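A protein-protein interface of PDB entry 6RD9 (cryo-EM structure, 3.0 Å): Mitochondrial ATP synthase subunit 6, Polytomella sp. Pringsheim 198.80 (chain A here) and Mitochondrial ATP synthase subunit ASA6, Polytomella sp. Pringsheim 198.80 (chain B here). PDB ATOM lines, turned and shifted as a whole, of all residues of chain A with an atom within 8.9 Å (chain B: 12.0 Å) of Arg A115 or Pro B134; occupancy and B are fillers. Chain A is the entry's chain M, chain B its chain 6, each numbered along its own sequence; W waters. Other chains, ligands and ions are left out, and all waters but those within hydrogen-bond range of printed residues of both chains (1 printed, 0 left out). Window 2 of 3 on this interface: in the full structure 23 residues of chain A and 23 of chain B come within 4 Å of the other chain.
The backbone carbonyl oxygen (O) of Ala B133 is in hydrogen-bond range of the side-chain hydroxyl (OG1) of Thr B136. The backbone carbonyl oxygen of Arg B130 lies within hydrogen-bond range of the backbone NH of Ala B137 (3.3 Å).
Among the printed residues, merely in contact across the chains: Asn A108 with Phe B129 (3.2 Å), Asn A108 with Ala B133 (3.4 Å), Asn A108 with Met B132 (3.6 Å), Asn A108 with Thr B136 (3.6 Å), Arg A115 with Pro B134 (3.7 Å), Gly A112 with Met B132 (3.7 Å), Phe A109 with Met B132 (3.9 Å) and Asn A108 with Arg B130 (3.9 Å).
Of the 18 printed residues of chain A, 4 touch a printed residue of chain B. Printed residues of chain A that touch a printed residue of chain B: Asn A108, Phe A109, Gly A112 and Arg A115. Hydrophobic or aromatic side chains of chain A within 4 Å of the printed part of chain B: Phe A109. Of the 17 printed residues of chain B, 6 touch a printed residue of chain A. Printed residues of chain B that touch a printed residue of chain A: Phe B129, Arg B130, Met B132, Ala B133, Pro B134 and Thr B136.
Of chain B, only Pro B134 comes within 4 Å of Arg A115. Pro B134 touches just one residue of chain A: Arg A115. Thr A111 touches none of the printed residues of chain B. Gly A112 touches one residue of chain B. No residue of chain B comes within 4 Å of Val A113. No residue of chain B comes within 4 Å of Tyr A114. No residue of chain B comes within 4 Å of Phe A116. Ala B133 touches one residue of chain A. Ala B135 touches none of the printed residues of chain A. Printed residues of chain B within 4 Å of Asn A108: Phe B129 (3.2 Å), Arg B130 (3.9 Å), Met B132 (3.6 Å), Ala B133 (3.4 Å) and Thr B136 (3.6 Å). Printed residues of chain A within 4 Å of Thr B136: Asn A108. Of the printed residues of chain A, Phe B129 touches Asn A108. Of the printed residues of chain A, Arg B130 touches Asn A108 (3.9 Å). Gln A120 touches none of the printed residues of chain B. The nearest residue of chain A that does not touch Pro B134 is Thr A111 (4.1 Å). The nearest printed residue of chain A that does not touch Met B132 is Val A113 (4.2 Å).
Water W1 lies within hydrogen-bond range of the backbone carbonyl oxygen (O) of Tyr B126 (3.1 Å) and the side-chain amide oxygen (OD1) of Asn A108 (3.4 Å).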
ATOM      1  N   THR A 107       9.799  12.703  -0.658  1.00  0.00           N
ATOM      2  CA  THR A 107      11.102  12.672  -1.302  1.00  0.00           C
ATOM      3  C   THR A 107      12.177  13.147  -0.350  1.00  0.00           C
ATOM      4  O   THR A 107      13.304  12.664  -0.390  1.00  0.00           O
ATOM      5  CB  THR A 107      11.046  13.544  -2.547  1.00  0.00           C
ATOM      6  OG1 THR A 107       9.944  13.130  -3.350  1.00  0.00           O
ATOM      7  CG2 THR A 107      12.279  13.445  -3.366  1.00  0.00           C
ATOM      8  N   ASN A 108      11.840  14.083   0.528  1.00  0.00           N
ATOM      9  CA  ASN A 108      12.801  14.593   1.492  1.00  0.00           C
ATOM     10  C   ASN A 108      12.985  13.641   2.653  1.00  0.00           C
ATOM     11  O   ASN A 108      14.065  13.567   3.229  1.00  0.00           O
ATOM     12  CB  ASN A 108      12.344  15.936   2.019  1.00  0.00           C
ATOM     13  CG  ASN A 108      12.323  16.973   0.988  1.00  0.00           C
ATOM     14  OD1 ASN A 108      11.579  17.929   1.089  1.00  0.00           O
ATOM     15  ND2 ASN A 108      13.117  16.798  -0.038  1.00  0.00           N
ATOM     16  N   PHE A 109      11.926  12.955   3.052  1.00  0.00           N
ATOM     17  CA  PHE A 109      12.047  11.981   4.120  1.00  0.00           C
ATOM     18  C   PHE A 109      12.850  10.778   3.664  1.00  0.00           C
ATOM     19  O   PHE A 109      13.822  10.400   4.311  1.00  0.00           O
ATOM     20  CB  PHE A 109      10.667  11.565   4.596  1.00  0.00           C
ATOM     21  CG  PHE A 109      10.685  10.552   5.683  1.00  0.00           C
ATOM     22  CD1 PHE A 109      11.152  10.875   6.932  1.00  0.00           C
ATOM     23  CD2 PHE A 109      10.207   9.283   5.467  1.00  0.00           C
ATOM     24  CE1 PHE A 109      11.163   9.954   7.926  1.00  0.00           C
ATOM     25  CE2 PHE A 109      10.223   8.360   6.461  1.00  0.00           C
ATOM     26  CZ  PHE A 109      10.701   8.699   7.689  1.00  0.00           C
ATOM     27  N   LEU A 110      12.504  10.202   2.519  1.00  0.00           N
ATOM     28  CA  LEU A 110      13.239   9.057   2.006  1.00  0.00           C
ATOM     29  C   LEU A 110      14.647   9.382   1.555  1.00  0.00           C
ATOM     30  O   LEU A 110      15.449   8.467   1.433  1.00  0.00           O
ATOM     31  CB  LEU A 110      12.500   8.419   0.844  1.00  0.00           C
ATOM     32  CG  LEU A 110      11.795   7.102   1.121  1.00  0.00           C
ATOM     33  CD1 LEU A 110      12.823   6.118   1.593  1.00  0.00           C
ATOM     34  CD2 LEU A 110      10.706   7.237   2.133  1.00  0.00           C
ATOM     35  N   THR A 111      14.965  10.634   1.258  1.00  0.00           N
ATOM     36  CA  THR A 111      16.355  10.997   1.021  1.00  0.00           C
ATOM     37  C   THR A 111      17.140  10.934   2.305  1.00  0.00           C
ATOM     38  O   THR A 111      18.239  10.392   2.344  1.00  0.00           O
ATOM     39  CB  THR A 111      16.454  12.396   0.455  1.00  0.00           C
ATOM     40  OG1 THR A 111      15.608  12.499  -0.680  1.00  0.00           O
ATOM     41  CG2 THR A 111      17.842  12.684   0.049  1.00  0.00           C
ATOM     42  N   GLY A 112      16.583  11.474   3.375  1.00  0.00           N
ATOM     43  CA  GLY A 112      17.272  11.441   4.639  1.00  0.00           C
ATOM     44  C   GLY A 112      17.320  10.069   5.250  1.00  0.00           C
ATOM     45  O   GLY A 112      18.247   9.758   5.987  1.00  0.00           O
ATOM     46  N   VAL A 113      16.331   9.233   4.962  1.00  0.00           N
ATOM     47  CA  VAL A 113      16.334   7.874   5.482  1.00  0.00           C
ATOM     48  C   VAL A 113      17.374   7.040   4.761  1.00  0.00           C
ATOM     49  O   VAL A 113      18.178   6.369   5.401  1.00  0.00           O
ATOM     50  CB  VAL A 113      14.934   7.259   5.380  1.00  0.00           C
ATOM     51  CG1 VAL A 113      14.986   5.805   5.619  1.00  0.00           C
ATOM     52  CG2 VAL A 113      14.045   7.867   6.374  1.00  0.00           C
ATOM     53  N   TYR A 114      17.413   7.111   3.431  1.00  0.00           N
ATOM     54  CA  TYR A 114      18.399   6.368   2.653  1.00  0.00           C
ATOM     55  C   TYR A 114      19.814   6.800   2.969  1.00  0.00           C
ATOM     56  O   TYR A 114      20.701   5.964   3.108  1.00  0.00           O
ATOM     57  CB  TYR A 114      18.158   6.548   1.158  1.00  0.00           C
ATOM     58  CG  TYR A 114      19.223   5.881   0.330  1.00  0.00           C
ATOM     59  CD1 TYR A 114      19.223   4.516   0.176  1.00  0.00           C
ATOM     60  CD2 TYR A 114      20.229   6.612  -0.289  1.00  0.00           C
ATOM     61  CE1 TYR A 114      20.172   3.902  -0.541  1.00  0.00           C
ATOM     62  CE2 TYR A 114      21.192   5.993  -1.002  1.00  0.00           C
ATOM     63  CZ  TYR A 114      21.158   4.638  -1.118  1.00  0.00           C
ATOM     64  OH  TYR A 114      22.114   4.000  -1.846  1.00  0.00           O
ATOM     65  N   ARG A 115      20.048   8.101   3.072  1.00  0.00           N
ATOM     66  CA  ARG A 115      21.369   8.608   3.389  1.00  0.00           C
ATOM     67  C   ARG A 115      21.776   8.314   4.813  1.00  0.00           C
ATOM     68  O   ARG A 115      22.956   8.419   5.128  1.00  0.00           O
ATOM     69  CB  ARG A 115      21.421  10.104   3.178  1.00  0.00           C
ATOM     70  CG  ARG A 115      21.453  10.504   1.766  1.00  0.00           C
ATOM     71  CD  ARG A 115      21.290  11.981   1.633  1.00  0.00           C
ATOM     72  NE  ARG A 115      22.331  12.704   2.327  1.00  0.00           N
ATOM     73  CZ  ARG A 115      23.518  12.967   1.811  1.00  0.00           C
ATOM     74  NH1 ARG A 115      24.410  13.632   2.510  1.00  0.00           N
ATOM     75  NH2 ARG A 115      23.820  12.558   0.600  1.00  0.00           N
ATOM     76  N   PHE A 116      20.830   7.993   5.684  1.00  0.00           N
ATOM     77  CA  PHE A 116      21.171   7.540   7.020  1.00  0.00           C
ATOM     78  C   PHE A 116      21.705   6.122   6.994  1.00  0.00           C
ATOM     79  O   PHE A 116      22.764   5.846   7.549  1.00  0.00           O
ATOM     80  CB  PHE A 116      19.960   7.624   7.929  1.00  0.00           C
ATOM     81  CG  PHE A 116      20.245   7.243   9.336  1.00  0.00           C
ATOM     82  CD1 PHE A 116      20.895   8.109  10.173  1.00  0.00           C
ATOM     83  CD2 PHE A 116      19.857   6.028   9.828  1.00  0.00           C
ATOM     84  CE1 PHE A 116      21.158   7.757  11.457  1.00  0.00           C
ATOM     85  CE2 PHE A 116      20.121   5.683  11.107  1.00  0.00           C
ATOM     86  CZ  PHE A 116      20.765   6.542  11.917  1.00  0.00           C
ATOM     87  N   TRP A 117      20.987   5.207   6.355  1.00  0.00           N
ATOM     88  CA  TRP A 117      21.398   3.815   6.369  1.00  0.00           C
ATOM     89  C   TRP A 117      22.590   3.572   5.487  1.00  0.00           C
ATOM     90  O   TRP A 117      23.327   2.612   5.700  1.00  0.00           O
ATOM     91  CB  TRP A 117      20.255   2.921   5.940  1.00  0.00           C
ATOM     92  CG  TRP A 117      19.094   3.055   6.786  1.00  0.00           C
ATOM     93  CD1 TRP A 117      17.912   3.544   6.433  1.00  0.00           C
ATOM     94  CD2 TRP A 117      18.987   2.685   8.149  1.00  0.00           C
ATOM     95  NE1 TRP A 117      17.059   3.533   7.481  1.00  0.00           N
ATOM     96  CE2 TRP A 117      17.707   3.007   8.558  1.00  0.00           C
ATOM     97  CE3 TRP A 117      19.863   2.134   9.071  1.00  0.00           C
ATOM     98  CZ2 TRP A 117      17.269   2.789   9.829  1.00  0.00           C
ATOM     99  CZ3 TRP A 117      19.434   1.928  10.316  1.00  0.00           C
ATOM    100  CH2 TRP A 117      18.149   2.253  10.695  1.00  0.00           C
ATOM    101  N   ARG A 118      22.795   4.421   4.497  1.00  0.00           N
ATOM    102  CA  ARG A 118      24.020   4.361   3.726  1.00  0.00           C
ATOM    103  C   ARG A 118      25.209   4.825   4.554  1.00  0.00           C
ATOM    104  O   ARG A 118      26.316   4.330   4.373  1.00  0.00           O
ATOM    105  CB  ARG A 118      23.822   5.175   2.459  1.00  0.00           C
ATOM    106  CG  ARG A 118      24.985   5.359   1.561  1.00  0.00           C
ATOM    107  CD  ARG A 118      25.677   4.082   1.210  1.00  0.00           C
ATOM    108  NE  ARG A 118      26.923   4.313   0.496  1.00  0.00           N
ATOM    109  CZ  ARG A 118      28.058   4.703   1.054  1.00  0.00           C
ATOM    110  NH1 ARG A 118      28.142   4.935   2.342  1.00  0.00           N
ATOM    111  NH2 ARG A 118      29.124   4.876   0.311  1.00  0.00           N
ATOM    112  N   SER A 119      24.997   5.712   5.509  1.00  0.00           N
ATOM    113  CA  SER A 119      26.082   6.207   6.335  1.00  0.00           C
ATOM    114  C   SER A 119      26.547   5.210   7.371  1.00  0.00           C
ATOM    115  O   SER A 119      27.537   5.469   8.048  1.00  0.00           O
ATOM    116  CB  SER A 119      25.652   7.467   7.053  1.00  0.00           C
ATOM    117  OG  SER A 119      24.744   7.154   8.075  1.00  0.00           O
ATOM    118  N   GLN A 120      25.850   4.098   7.533  1.00  0.00           N
ATOM    119  CA  GLN A 120      26.200   3.159   8.579  1.00  0.00           C
ATOM    120  C   GLN A 120      27.361   2.282   8.181  1.00  0.00           C
ATOM    121  O   GLN A 120      28.116   1.840   9.044  1.00  0.00           O
ATOM    122  CB  GLN A 120      25.004   2.299   8.934  1.00  0.00           C
ATOM    123  CG  GLN A 120      23.802   3.048   9.399  1.00  0.00           C
ATOM    124  CD  GLN A 120      24.057   3.853  10.617  1.00  0.00           C
ATOM    125  OE1 GLN A 120      23.714   5.016  10.687  1.00  0.00           O
ATOM    126  NE2 GLN A 120      24.665   3.243  11.594  1.00  0.00           N
ATOM    127  N   ASN A 121      27.527   2.015   6.900  1.00  0.00           N
ATOM    128  CA  ASN A 121      28.695   1.316   6.388  1.00  0.00           C
ATOM    129  C   ASN A 121      29.382   2.230   5.395  1.00  0.00           C
ATOM    130  O   ASN A 121      29.175   2.104   4.186  1.00  0.00           O
ATOM    131  CB  ASN A 121      28.311   0.007   5.719  1.00  0.00           C
ATOM    132  CG  ASN A 121      27.359  -0.790   6.532  1.00  0.00           C
ATOM    133  OD1 ASN A 121      26.206  -0.926   6.171  1.00  0.00           O
ATOM    134  ND2 ASN A 121      27.830  -1.340   7.630  1.00  0.00           N
ATOM    135  N   GLY A 149      22.879   0.071   2.066  1.00  0.00           N
ATOM    136  CA  GLY A 149      22.125   1.297   2.139  1.00  0.00           C
ATOM    137  C   GLY A 149      20.724   1.144   1.623  1.00  0.00           C
ATOM    138  O   GLY A 149      19.811   1.758   2.152  1.00  0.00           O
ATOM    139  N   THR A 150      20.532   0.299   0.618  1.00  0.00           N
ATOM    140  CA  THR A 150      19.228   0.000   0.045  1.00  0.00           C
ATOM    141  C   THR A 150      18.501  -1.072   0.826  1.00  0.00           C
ATOM    142  O   THR A 150      17.284  -0.999   0.991  1.00  0.00           O
ATOM    143  CB  THR A 150      19.384  -0.461  -1.400  1.00  0.00           C
ATOM    144  OG1 THR A 150      20.214   0.453  -2.109  1.00  0.00           O
ATOM    145  CG2 THR A 150      18.071  -0.529  -2.088  1.00  0.00           C
ATOM    146  N   THR A 153      17.156   0.318   4.284  1.00  0.00           N
ATOM    147  CA  THR A 153      15.983   1.167   4.178  1.00  0.00           C
ATOM    148  C   THR A 153      14.817   0.440   3.556  1.00  0.00           C
ATOM    149  O   THR A 153      13.709   0.957   3.575  1.00  0.00           O
ATOM    150  CB  THR A 153      16.284   2.448   3.403  1.00  0.00           C
ATOM    151  OG1 THR A 153      15.102   3.228   3.289  1.00  0.00           O
ATOM    152  CG2 THR A 153      16.681   2.163   2.099  1.00  0.00           C
ATOM    153  N   TYR B 126       7.448  19.909   8.828  1.00  0.00           N
ATOM    154  CA  TYR B 126       7.647  20.090   7.396  1.00  0.00           C
ATOM    155  C   TYR B 126       9.016  20.665   7.103  1.00  0.00           C
ATOM    156  O   TYR B 126       9.687  20.243   6.164  1.00  0.00           O
ATOM    157  CB  TYR B 126       6.571  21.002   6.829  1.00  0.00           C
ATOM    158  CG  TYR B 126       6.762  21.324   5.379  1.00  0.00           C
ATOM    159  CD1 TYR B 126       6.428  20.412   4.409  1.00  0.00           C
ATOM    160  CD2 TYR B 126       7.272  22.539   4.977  1.00  0.00           C
ATOM    161  CE1 TYR B 126       6.612  20.691   3.098  1.00  0.00           C
ATOM    162  CE2 TYR B 126       7.464  22.817   3.670  1.00  0.00           C
ATOM    163  CZ  TYR B 126       7.127  21.890   2.739  1.00  0.00           C
ATOM    164  OH  TYR B 126       7.310  22.169   1.423  1.00  0.00           O
ATOM    165  N   PHE B 127       9.449  21.632   7.887  1.00  0.00           N
ATOM    166  CA  PHE B 127      10.752  22.225   7.664  1.00  0.00           C
ATOM    167  C   PHE B 127      11.867  21.408   8.267  1.00  0.00           C
ATOM    168  O   PHE B 127      13.031  21.688   7.987  1.00  0.00           O
ATOM    169  CB  PHE B 127      10.786  23.637   8.224  1.00  0.00           C
ATOM    170  CG  PHE B 127      10.182  24.646   7.322  1.00  0.00           C
ATOM    171  CD1 PHE B 127      10.893  25.148   6.270  1.00  0.00           C
ATOM    172  CD2 PHE B 127       8.897  25.079   7.514  1.00  0.00           C
ATOM    173  CE1 PHE B 127      10.330  26.058   5.433  1.00  0.00           C
ATOM    174  CE2 PHE B 127       8.340  25.986   6.683  1.00  0.00           C
ATOM    175  CZ  PHE B 127       9.054  26.475   5.646  1.00  0.00           C
ATOM    176  N   ALA B 128      11.551  20.421   9.088  1.00  0.00           N
ATOM    177  CA  ALA B 128      12.553  19.488   9.564  1.00  0.00           C
ATOM    178  C   ALA B 128      12.799  18.369   8.586  1.00  0.00           C
ATOM    179  O   ALA B 128      13.883  17.796   8.590  1.00  0.00           O
ATOM    180  CB  ALA B 128      12.143  18.883  10.897  1.00  0.00           C
ATOM    181  N   PHE B 129      11.812  18.013   7.777  1.00  0.00           N
ATOM    182  CA  PHE B 129      12.057  17.035   6.728  1.00  0.00           C
ATOM    183  C   PHE B 129      12.749  17.679   5.552  1.00  0.00           C
ATOM    184  O   PHE B 129      13.474  17.008   4.826  1.00  0.00           O
ATOM    185  CB  PHE B 129      10.763  16.381   6.269  1.00  0.00           C
ATOM    186  CG  PHE B 129      10.178  15.416   7.259  1.00  0.00           C
ATOM    187  CD1 PHE B 129      10.870  15.017   8.372  1.00  0.00           C
ATOM    188  CD2 PHE B 129       8.928  14.910   7.068  1.00  0.00           C
ATOM    189  CE1 PHE B 129      10.325  14.153   9.255  1.00  0.00           C
ATOM    190  CE2 PHE B 129       8.390  14.037   7.948  1.00  0.00           C
ATOM    191  CZ  PHE B 129       9.088  13.663   9.040  1.00  0.00           C
ATOM    192  N   ARG B 130      12.561  18.980   5.361  1.00  0.00           N
ATOM    193  CA  ARG B 130      13.281  19.707   4.329  1.00  0.00           C
ATOM    194  C   ARG B 130      14.761  19.800   4.612  1.00  0.00           C
ATOM    195  O   ARG B 130      15.532  20.017   3.684  1.00  0.00           O
ATOM    196  CB  ARG B 130      12.726  21.107   4.185  1.00  0.00           C
ATOM    197  CG  ARG B 130      11.550  21.177   3.313  1.00  0.00           C
ATOM    198  CD  ARG B 130      11.142  22.585   3.083  1.00  0.00           C
ATOM    199  NE  ARG B 130      12.007  23.253   2.138  1.00  0.00           N
ATOM    200  CZ  ARG B 130      11.753  23.342   0.846  1.00  0.00           C
ATOM    201  NH1 ARG B 130      10.673  22.797   0.351  1.00  0.00           N
ATOM    202  NH2 ARG B 130      12.589  23.965   0.050  1.00  0.00           N
ATOM    203  N   GLY B 131      15.172  19.681   5.857  1.00  0.00           N
ATOM    204  CA  GLY B 131      16.573  19.629   6.188  1.00  0.00           C
ATOM    205  C   GLY B 131      17.185  18.262   6.148  1.00  0.00           C
ATOM    206  O   GLY B 131      18.402  18.148   6.223  1.00  0.00           O
ATOM    207  N   MET B 132      16.376  17.213   6.043  1.00  0.00           N
ATOM    208  CA  MET B 132      16.921  15.872   5.887  1.00  0.00           C
ATOM    209  C   MET B 132      17.523  15.686   4.513  1.00  0.00           C
ATOM    210  O   MET B 132      18.488  14.938   4.347  1.00  0.00           O
ATOM    211  CB  MET B 132      15.841  14.819   6.092  1.00  0.00           C
ATOM    212  CG  MET B 132      15.097  14.885   7.355  1.00  0.00           C
ATOM    213  SD  MET B 132      13.941  13.541   7.439  1.00  0.00           S
ATOM    214  CE  MET B 132      15.074  12.193   7.609  1.00  0.00           C
ATOM    215  N   ALA B 133      16.964  16.284   3.562  1.00  0.00           N
ATOM    216  CA  ALA B 133      17.402  16.224   2.189  1.00  0.00           C
ATOM    217  C   ALA B 133      18.363  17.350   1.916  1.00  0.00           C
ATOM    218  O   ALA B 133      18.015  18.504   2.142  1.00  0.00           O
ATOM    219  CB  ALA B 133      16.224  16.349   1.260  1.00  0.00           C
ATOM    220  N   PRO B 134      19.564  17.078   1.411  1.00  0.00           N
ATOM    221  CA  PRO B 134      20.465  18.168   1.043  1.00  0.00           C
ATOM    222  C   PRO B 134      19.991  18.991  -0.131  1.00  0.00           C
ATOM    223  O   PRO B 134      20.503  20.092  -0.320  1.00  0.00           O
ATOM    224  CB  PRO B 134      21.762  17.438   0.706  1.00  0.00           C
ATOM    225  CG  PRO B 134      21.650  16.177   1.335  1.00  0.00           C
ATOM    226  CD  PRO B 134      20.237  15.788   1.291  1.00  0.00           C
ATOM    227  N   ALA B 135      19.034  18.501  -0.915  1.00  0.00           N
ATOM    228  CA  ALA B 135      18.491  19.258  -2.029  1.00  0.00           C
ATOM    229  C   ALA B 135      17.626  20.412  -1.572  1.00  0.00           C
ATOM    230  O   ALA B 135      17.470  21.391  -2.301  1.00  0.00           O
ATOM    231  CB  ALA B 135      17.677  18.346  -2.920  1.00  0.00           C
ATOM    232  N   THR B 136      17.026  20.315  -0.402  1.00  0.00           N
ATOM    233  CA  THR B 136      16.160  21.359   0.107  1.00  0.00           C
ATOM    234  C   THR B 136      16.732  22.033   1.336  1.00  0.00           C
ATOM    235  O   THR B 136      16.166  23.011   1.809  1.00  0.00           O
ATOM    236  CB  THR B 136      14.794  20.787   0.439  1.00  0.00           C
ATOM    237  OG1 THR B 136      14.965  19.751   1.392  1.00  0.00           O
ATOM    238  CG2 THR B 136      14.162  20.193  -0.748  1.00  0.00           C
ATOM    239  N   ALA B 137      17.829  21.529   1.867  1.00  0.00           N
ATOM    240  CA  ALA B 137      18.484  22.136   3.002  1.00  0.00           C
ATOM    241  C   ALA B 137      19.265  23.387   2.640  1.00  0.00           C
ATOM    242  O   ALA B 137      19.695  24.106   3.543  1.00  0.00           O
ATOM    243  CB  ALA B 137      19.415  21.125   3.655  1.00  0.00           C
ATOM    244  N   SER B 138      19.459  23.668   1.357  1.00  0.00           N
ATOM    245  CA  SER B 138      20.216  24.821   0.909  1.00  0.00           C
ATOM    246  C   SER B 138      19.506  25.402  -0.297  1.00  0.00           C
ATOM    247  O   SER B 138      18.399  24.995  -0.644  1.00  0.00           O
ATOM    248  CB  SER B 138      21.651  24.425   0.564  1.00  0.00           C
ATOM    249  OG  SER B 138      22.314  23.900   1.684  1.00  0.00           O
ATOM    250  N   THR B 139      20.151  26.359  -0.944  1.00  0.00           N
ATOM    251  CA  THR B 139      19.706  26.916  -2.206  1.00  0.00           C
ATOM    252  C   THR B 139      20.623  26.363  -3.284  1.00  0.00           C
ATOM    253  O   THR B 139      21.735  25.933  -2.983  1.00  0.00           O
ATOM    254  CB  THR B 139      19.785  28.440  -2.154  1.00  0.00           C
ATOM    255  OG1 THR B 139      19.294  28.879  -0.890  1.00  0.00           O
ATOM    256  CG2 THR B 139      18.903  29.086  -3.212  1.00  0.00           C
ATOM    257  N   LEU B 140      20.161  26.346  -4.531  1.00  0.00           N
ATOM    258  CA  LEU B 140      21.043  25.988  -5.629  1.00  0.00           C
ATOM    259  C   LEU B 140      22.186  26.975  -5.768  1.00  0.00           C
ATOM    260  O   LEU B 140      22.066  28.149  -5.438  1.00  0.00           O
ATOM    261  CB  LEU B 140      20.298  25.928  -6.940  1.00  0.00           C
ATOM    262  CG  LEU B 140      19.743  24.591  -7.310  1.00  0.00           C
ATOM    263  CD1 LEU B 140      19.161  24.805  -8.601  1.00  0.00           C
ATOM    264  CD2 LEU B 140      20.868  23.656  -7.448  1.00  0.00           C
ATOM    265  N   ASN B 141      23.299  26.493  -6.296  1.00  0.00           N
ATOM    266  CA  ASN B 141      24.540  27.191  -6.098  1.00  0.00           C
ATOM    267  C   ASN B 141      25.313  27.560  -7.349  1.00  0.00           C
ATOM    268  O   ASN B 141      26.237  28.365  -7.242  1.00  0.00           O
ATOM    269  CB  ASN B 141      25.464  26.375  -5.205  1.00  0.00           C
ATOM    270  CG  ASN B 141      26.372  27.234  -4.396  1.00  0.00           C
ATOM    271  OD1 ASN B 141      26.062  28.389  -4.136  1.00  0.00           O
ATOM    272  ND2 ASN B 141      27.513  26.688  -4.004  1.00  0.00           N
ATOM    273  N   GLY B 142      25.004  27.034  -8.512  1.00  0.00           N
ATOM    274  CA  GLY B 142      25.818  27.364  -9.663  1.00  0.00           C
ATOM    275  C   GLY B 142      25.501  28.711 -10.260  1.00  0.00           C
ATOM    276  O   GLY B 142      24.715  29.478  -9.721  1.00  0.00           O
HETATM  277  O   HOH W   1       9.311  18.760   3.509  1.00  0.00           O
